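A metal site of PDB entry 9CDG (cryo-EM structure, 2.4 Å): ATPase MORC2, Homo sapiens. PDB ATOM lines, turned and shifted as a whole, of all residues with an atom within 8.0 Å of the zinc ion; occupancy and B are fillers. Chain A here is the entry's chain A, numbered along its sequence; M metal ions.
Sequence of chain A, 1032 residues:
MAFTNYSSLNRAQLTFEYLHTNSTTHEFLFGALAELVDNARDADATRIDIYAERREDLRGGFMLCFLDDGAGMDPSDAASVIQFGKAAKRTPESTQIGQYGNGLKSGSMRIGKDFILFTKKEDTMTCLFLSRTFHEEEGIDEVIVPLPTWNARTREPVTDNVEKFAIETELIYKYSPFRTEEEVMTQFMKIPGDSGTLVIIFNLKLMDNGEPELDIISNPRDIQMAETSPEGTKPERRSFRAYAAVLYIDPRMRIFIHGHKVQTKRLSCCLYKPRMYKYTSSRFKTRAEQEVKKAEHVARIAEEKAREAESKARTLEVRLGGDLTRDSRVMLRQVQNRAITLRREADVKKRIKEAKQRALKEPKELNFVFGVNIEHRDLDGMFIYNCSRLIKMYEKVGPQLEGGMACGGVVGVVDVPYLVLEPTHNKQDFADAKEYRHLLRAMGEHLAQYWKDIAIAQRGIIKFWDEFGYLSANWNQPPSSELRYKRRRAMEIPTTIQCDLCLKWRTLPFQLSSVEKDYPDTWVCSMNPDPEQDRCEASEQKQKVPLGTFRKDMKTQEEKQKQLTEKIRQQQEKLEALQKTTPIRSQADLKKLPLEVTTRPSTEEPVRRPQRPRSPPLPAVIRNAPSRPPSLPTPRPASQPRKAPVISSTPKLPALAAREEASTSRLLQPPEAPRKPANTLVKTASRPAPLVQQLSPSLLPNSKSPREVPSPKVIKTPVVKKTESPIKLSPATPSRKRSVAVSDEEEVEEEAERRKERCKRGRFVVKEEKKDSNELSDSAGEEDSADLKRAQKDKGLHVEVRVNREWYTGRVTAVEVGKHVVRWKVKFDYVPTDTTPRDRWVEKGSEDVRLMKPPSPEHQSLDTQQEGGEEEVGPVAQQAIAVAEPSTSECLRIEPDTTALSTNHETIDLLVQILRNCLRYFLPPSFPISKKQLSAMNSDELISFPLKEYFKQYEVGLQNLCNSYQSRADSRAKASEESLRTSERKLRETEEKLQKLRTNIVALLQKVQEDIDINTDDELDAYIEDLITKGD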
ATOM      1  N   GLN A 498     -28.070   9.292 -24.857  1.00  0.00           N
ATOM      2  CA  GLN A 498     -28.392   8.618 -26.108  1.00  0.00           C
ATOM      3  C   GLN A 498     -27.366   7.560 -26.471  1.00  0.00           C
ATOM      4  O   GLN A 498     -26.163   7.746 -26.271  1.00  0.00           O
ATOM      5  CB  GLN A 498     -28.481   9.650 -27.239  1.00  0.00           C
ATOM      6  CG  GLN A 498     -29.031   9.121 -28.550  1.00  0.00           C
ATOM      7  CD  GLN A 498     -29.090  10.189 -29.625  1.00  0.00           C
ATOM      8  OE1 GLN A 498     -28.401  11.196 -29.561  1.00  0.00           O
ATOM      9  NE2 GLN A 498     -29.926   9.949 -30.634  1.00  0.00           N
ATOM     10  N   CYS A 499     -27.845   6.436 -27.002  1.00  0.00           N
ATOM     11  CA  CYS A 499     -26.964   5.418 -27.546  1.00  0.00           C
ATOM     12  C   CYS A 499     -26.388   5.873 -28.888  1.00  0.00           C
ATOM     13  O   CYS A 499     -26.877   6.802 -29.526  1.00  0.00           O
ATOM     14  CB  CYS A 499     -27.708   4.100 -27.723  1.00  0.00           C
ATOM     15  SG  CYS A 499     -26.901   2.943 -28.861  1.00  0.00           S
ATOM     16  N   ASP A 500     -25.323   5.190 -29.321  1.00  0.00           N
ATOM     17  CA  ASP A 500     -24.593   5.591 -30.510  1.00  0.00           C
ATOM     18  C   ASP A 500     -25.014   4.858 -31.776  1.00  0.00           C
ATOM     19  O   ASP A 500     -24.862   5.419 -32.867  1.00  0.00           O
ATOM     20  CB  ASP A 500     -23.088   5.382 -30.303  1.00  0.00           C
ATOM     21  CG  ASP A 500     -22.410   6.597 -29.702  1.00  0.00           C
ATOM     22  OD1 ASP A 500     -22.024   7.498 -30.482  1.00  0.00           O
ATOM     23  OD2 ASP A 500     -22.274   6.660 -28.470  1.00  0.00           O
ATOM     24  N   LEU A 501     -25.522   3.636 -31.685  1.00  0.00           N
ATOM     25  CA  LEU A 501     -25.880   2.876 -32.876  1.00  0.00           C
ATOM     26  C   LEU A 501     -27.356   3.045 -33.235  1.00  0.00           C
ATOM     27  O   LEU A 501     -27.694   3.482 -34.334  1.00  0.00           O
ATOM     28  CB  LEU A 501     -25.535   1.383 -32.732  1.00  0.00           C
ATOM     29  CG  LEU A 501     -24.218   0.839 -32.170  1.00  0.00           C
ATOM     30  CD1 LEU A 501     -24.142   0.831 -30.646  1.00  0.00           C
ATOM     31  CD2 LEU A 501     -23.965  -0.552 -32.714  1.00  0.00           C
ATOM     32  N   CYS A 502     -28.251   2.678 -32.311  1.00  0.00           N
ATOM     33  CA  CYS A 502     -29.680   2.783 -32.577  1.00  0.00           C
ATOM     34  C   CYS A 502     -30.229   4.181 -32.334  1.00  0.00           C
ATOM     35  O   CYS A 502     -31.412   4.416 -32.629  1.00  0.00           O
ATOM     36  CB  CYS A 502     -30.457   1.781 -31.728  1.00  0.00           C
ATOM     37  SG  CYS A 502     -30.411   2.134 -29.958  1.00  0.00           S
ATOM     38  N   LEU A 503     -29.414   5.085 -31.765  1.00  0.00           N
ATOM     39  CA  LEU A 503     -29.728   6.495 -31.532  1.00  0.00           C
ATOM     40  C   LEU A 503     -30.918   6.695 -30.595  1.00  0.00           C
ATOM     41  O   LEU A 503     -31.517   7.777 -30.578  1.00  0.00           O
ATOM     42  CB  LEU A 503     -29.964   7.262 -32.839  1.00  0.00           C
ATOM     43  CG  LEU A 503     -28.854   7.148 -33.879  1.00  0.00           C
ATOM     44  CD1 LEU A 503     -29.379   7.541 -35.235  1.00  0.00           C
ATOM     45  CD2 LEU A 503     -27.688   8.033 -33.486  1.00  0.00           C
ATOM     46  N   LYS A 504     -31.264   5.696 -29.797  1.00  0.00           N
ATOM     47  CA  LYS A 504     -32.388   5.822 -28.886  1.00  0.00           C
ATOM     48  C   LYS A 504     -31.947   6.534 -27.612  1.00  0.00           C
ATOM     49  O   LYS A 504     -30.778   6.519 -27.229  1.00  0.00           O
ATOM     50  CB  LYS A 504     -32.979   4.457 -28.559  1.00  0.00           C
ATOM     51  CG  LYS A 504     -33.722   3.817 -29.727  1.00  0.00           C
ATOM     52  CD  LYS A 504     -34.222   2.431 -29.385  1.00  0.00           C
ATOM     53  CE  LYS A 504     -34.674   1.692 -30.623  1.00  0.00           C
ATOM     54  NZ  LYS A 504     -35.307   0.387 -30.294  1.00  0.00           N
ATOM     55  N   TRP A 505     -32.915   7.149 -26.944  1.00  0.00           N
ATOM     56  CA  TRP A 505     -32.666   7.910 -25.732  1.00  0.00           C
ATOM     57  C   TRP A 505     -33.018   7.050 -24.524  1.00  0.00           C
ATOM     58  O   TRP A 505     -34.182   6.656 -24.356  1.00  0.00           O
ATOM     59  CB  TRP A 505     -33.460   9.211 -25.739  1.00  0.00           C
ATOM     60  CG  TRP A 505     -32.907  10.218 -26.684  1.00  0.00           C
ATOM     61  CD1 TRP A 505     -33.320  10.443 -27.965  1.00  0.00           C
ATOM     62  CD2 TRP A 505     -31.833  11.121 -26.430  1.00  0.00           C
ATOM     63  NE1 TRP A 505     -32.559  11.445 -28.525  1.00  0.00           N
ATOM     64  CE2 TRP A 505     -31.650  11.874 -27.597  1.00  0.00           C
ATOM     65  CE3 TRP A 505     -31.022  11.372 -25.322  1.00  0.00           C
ATOM     66  CZ2 TRP A 505     -30.673  12.860 -27.696  1.00  0.00           C
ATOM     67  CZ3 TRP A 505     -30.059  12.358 -25.422  1.00  0.00           C
ATOM     68  CH2 TRP A 505     -29.889  13.078 -26.603  1.00  0.00           C
ATOM     69  N   ARG A 506     -32.025   6.774 -23.689  1.00  0.00           N
ATOM     70  CA  ARG A 506     -32.194   5.918 -22.526  1.00  0.00           C
ATOM     71  C   ARG A 506     -32.044   6.734 -21.255  1.00  0.00           C
ATOM     72  O   ARG A 506     -31.274   7.697 -21.213  1.00  0.00           O
ATOM     73  CB  ARG A 506     -31.177   4.774 -22.536  1.00  0.00           C
ATOM     74  CG  ARG A 506     -31.111   4.016 -23.840  1.00  0.00           C
ATOM     75  CD  ARG A 506     -32.440   3.359 -24.162  1.00  0.00           C
ATOM     76  NE  ARG A 506     -32.308   2.310 -25.158  1.00  0.00           N
ATOM     77  CZ  ARG A 506     -33.319   1.688 -25.736  1.00  0.00           C
ATOM     78  NH1 ARG A 506     -34.576   1.996 -25.455  1.00  0.00           N
ATOM     79  NH2 ARG A 506     -33.076   0.742 -26.632  1.00  0.00           N
ATOM     80  N   TRP A 523     -21.422   5.968 -25.762  1.00  0.00           N
ATOM     81  CA  TRP A 523     -22.277   5.152 -24.906  1.00  0.00           C
ATOM     82  C   TRP A 523     -23.177   4.271 -25.749  1.00  0.00           C
ATOM     83  O   TRP A 523     -23.707   4.703 -26.773  1.00  0.00           O
ATOM     84  CB  TRP A 523     -23.114   6.031 -23.981  1.00  0.00           C
ATOM     85  CG  TRP A 523     -23.838   5.265 -22.938  1.00  0.00           C
ATOM     86  CD1 TRP A 523     -23.379   4.927 -21.696  1.00  0.00           C
ATOM     87  CD2 TRP A 523     -25.162   4.724 -23.029  1.00  0.00           C
ATOM     88  NE1 TRP A 523     -24.336   4.224 -21.014  1.00  0.00           N
ATOM     89  CE2 TRP A 523     -25.442   4.084 -21.807  1.00  0.00           C
ATOM     90  CE3 TRP A 523     -26.139   4.741 -24.024  1.00  0.00           C
ATOM     91  CZ2 TRP A 523     -26.653   3.457 -21.554  1.00  0.00           C
ATOM     92  CZ3 TRP A 523     -27.350   4.114 -23.772  1.00  0.00           C
ATOM     93  CH2 TRP A 523     -27.595   3.480 -22.547  1.00  0.00           C
ATOM     94  N   VAL A 524     -23.330   3.030 -25.305  1.00  0.00           N
ATOM     95  CA  VAL A 524     -24.096   2.012 -26.006  1.00  0.00           C
ATOM     96  C   VAL A 524     -25.208   1.574 -25.045  1.00  0.00           C
ATOM     97  O   VAL A 524     -25.084   1.720 -23.835  1.00  0.00           O
ATOM     98  CB  VAL A 524     -23.181   0.851 -26.479  1.00  0.00           C
ATOM     99  CG1 VAL A 524     -23.894  -0.321 -27.146  1.00  0.00           C
ATOM    100  CG2 VAL A 524     -22.085   1.369 -27.411  1.00  0.00           C
ATOM    101  N   CYS A 525     -26.321   1.080 -25.593  1.00  0.00           N
ATOM    102  CA  CYS A 525     -27.426   0.585 -24.772  1.00  0.00           C
ATOM    103  C   CYS A 525     -27.054  -0.626 -23.908  1.00  0.00           C
ATOM    104  O   CYS A 525     -27.800  -0.930 -22.975  1.00  0.00           O
ATOM    105  CB  CYS A 525     -28.624   0.238 -25.646  1.00  0.00           C
ATOM    106  SG  CYS A 525     -29.474   1.675 -26.335  1.00  0.00           S
ATOM    107  N   SER A 526     -25.948  -1.319 -24.200  1.00  0.00           N
ATOM    108  CA  SER A 526     -25.552  -2.497 -23.436  1.00  0.00           C
ATOM    109  C   SER A 526     -25.166  -2.185 -21.994  1.00  0.00           C
ATOM    110  O   SER A 526     -25.535  -2.954 -21.090  1.00  0.00           O
ATOM    111  CB  SER A 526     -24.397  -3.212 -24.132  1.00  0.00           C
ATOM    112  OG  SER A 526     -24.527  -3.145 -25.542  1.00  0.00           O
ATOM    113  N   GLN A 533     -34.133  -1.951 -20.449  1.00  0.00           N
ATOM    114  CA  GLN A 533     -33.616  -1.247 -21.622  1.00  0.00           C
ATOM    115  C   GLN A 533     -32.112  -1.429 -21.743  1.00  0.00           C
ATOM    116  O   GLN A 533     -31.356  -0.477 -21.980  1.00  0.00           O
ATOM    117  CB  GLN A 533     -33.975   0.232 -21.556  1.00  0.00           C
ATOM    118  CG  GLN A 533     -34.105   0.765 -20.139  1.00  0.00           C
ATOM    119  CD  GLN A 533     -34.257   2.273 -20.081  1.00  0.00           C
ATOM    120  OE1 GLN A 533     -33.280   3.010 -20.272  1.00  0.00           O
ATOM    121  NE2 GLN A 533     -35.466   2.745 -19.837  1.00  0.00           N
ATOM    122  N   ASP A 534     -31.640  -2.656 -21.571  1.00  0.00           N
ATOM    123  CA  ASP A 534     -30.221  -2.954 -21.703  1.00  0.00           C
ATOM    124  C   ASP A 534     -29.821  -3.350 -23.117  1.00  0.00           C
ATOM    125  O   ASP A 534     -28.655  -3.714 -23.341  1.00  0.00           O
ATOM    126  CB  ASP A 534     -29.802  -4.067 -20.735  1.00  0.00           C
ATOM    127  CG  ASP A 534     -30.831  -5.172 -20.623  1.00  0.00           C
ATOM    128  OD1 ASP A 534     -31.533  -5.450 -21.619  1.00  0.00           O
ATOM    129  OD2 ASP A 534     -30.912  -5.796 -19.540  1.00  0.00           O
ATOM    130  N   ARG A 535     -30.738  -3.303 -24.072  1.00  0.00           N
ATOM    131  CA  ARG A 535     -30.457  -3.711 -25.433  1.00  0.00           C
ATOM    132  C   ARG A 535     -30.910  -2.621 -26.409  1.00  0.00           C
ATOM    133  O   ARG A 535     -31.748  -1.785 -26.094  1.00  0.00           O
ATOM    134  CB  ARG A 535     -31.135  -5.051 -25.774  1.00  0.00           C
ATOM    135  CG  ARG A 535     -32.616  -4.956 -26.084  1.00  0.00           C
ATOM    136  CD  ARG A 535     -33.342  -6.224 -25.681  1.00  0.00           C
ATOM    137  NE  ARG A 535     -33.279  -6.465 -24.246  1.00  0.00           N
ATOM    138  CZ  ARG A 535     -34.114  -5.931 -23.357  1.00  0.00           C
ATOM    139  NH1 ARG A 535     -35.108  -5.146 -23.730  1.00  0.00           N
ATOM    140  NH2 ARG A 535     -33.944  -6.205 -22.068  1.00  0.00           N
ATOM    141  N   CYS A 536     -30.297  -2.639 -27.596  1.00  0.00           N
ATOM    142  CA  CYS A 536     -30.638  -1.660 -28.625  1.00  0.00           C
ATOM    143  C   CYS A 536     -31.939  -1.992 -29.337  1.00  0.00           C
ATOM    144  O   CYS A 536     -32.511  -1.125 -29.999  1.00  0.00           O
ATOM    145  CB  CYS A 536     -29.508  -1.558 -29.645  1.00  0.00           C
ATOM    146  SG  CYS A 536     -28.050  -0.675 -29.046  1.00  0.00           S
ATOM    147  N   GLU A 537     -32.420  -3.226 -29.229  1.00  0.00           N
ATOM    148  CA  GLU A 537     -33.685  -3.637 -29.814  1.00  0.00           C
ATOM    149  C   GLU A 537     -34.878  -3.323 -28.916  1.00  0.00           C
ATOM    150  O   GLU A 537     -36.019  -3.587 -29.308  1.00  0.00           O
ATOM    151  CB  GLU A 537     -33.676  -5.131 -30.129  1.00  0.00           C
ATOM    152  CG  GLU A 537     -32.389  -5.612 -30.778  1.00  0.00           C
ATOM    153  CD  GLU A 537     -32.211  -5.081 -32.190  1.00  0.00           C
ATOM    154  OE1 GLU A 537     -33.223  -4.944 -32.908  1.00  0.00           O
ATOM    155  OE2 GLU A 537     -31.059  -4.794 -32.580  1.00  0.00           O
ATOM    156  N   ALA A 538     -34.642  -2.756 -27.730  1.00  0.00           N
ATOM    157  CA  ALA A 538     -35.702  -2.447 -26.807  1.00  0.00           C
ATOM    158  C   ALA A 538     -36.518  -1.252 -27.297  1.00  0.00           C
ATOM    159  O   ALA A 538     -36.060  -0.446 -28.097  1.00  0.00           O
ATOM    160  CB  ALA A 538     -35.141  -2.154 -25.414  1.00  0.00           C
HETATM  161 ZN    ZN M   1     -28.701   1.504 -28.524  1.00  0.00          ZN
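N of Leu 501 lies close to SG of Cys 499 (3.2 Å).
The backbone carbonyl oxygen of Cys 536 lies within hydrogen-bond range of the side-chain amino group of Lys 504, 3.2 Å away.
The side-chain sulfur (SG) of Cys 525 lies close to the guanidinium group (NE) of Arg 506.
SG of Cys 502 lies close to N of Lys 504 (3.7 Å).
The backbone NH of Cys 499 is in hydrogen-bond range of the backbone carbonyl oxygen of Lys 504.
Four residues have an atom within 4 Å of the zinc ion: Cys 499, Cys 502, Cys 525 and Cys 536.
The zinc ion is bound by the side-chain sulfur (SG) of Cys 502 (2.3 Å), the side-chain sulfur (SG) of Cys 525 (2.3 Å), the side-chain sulfur (SG) of Cys 499 (2.3 Å) and the side-chain sulfur (SG) of Cys 536 (2.3 Å).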
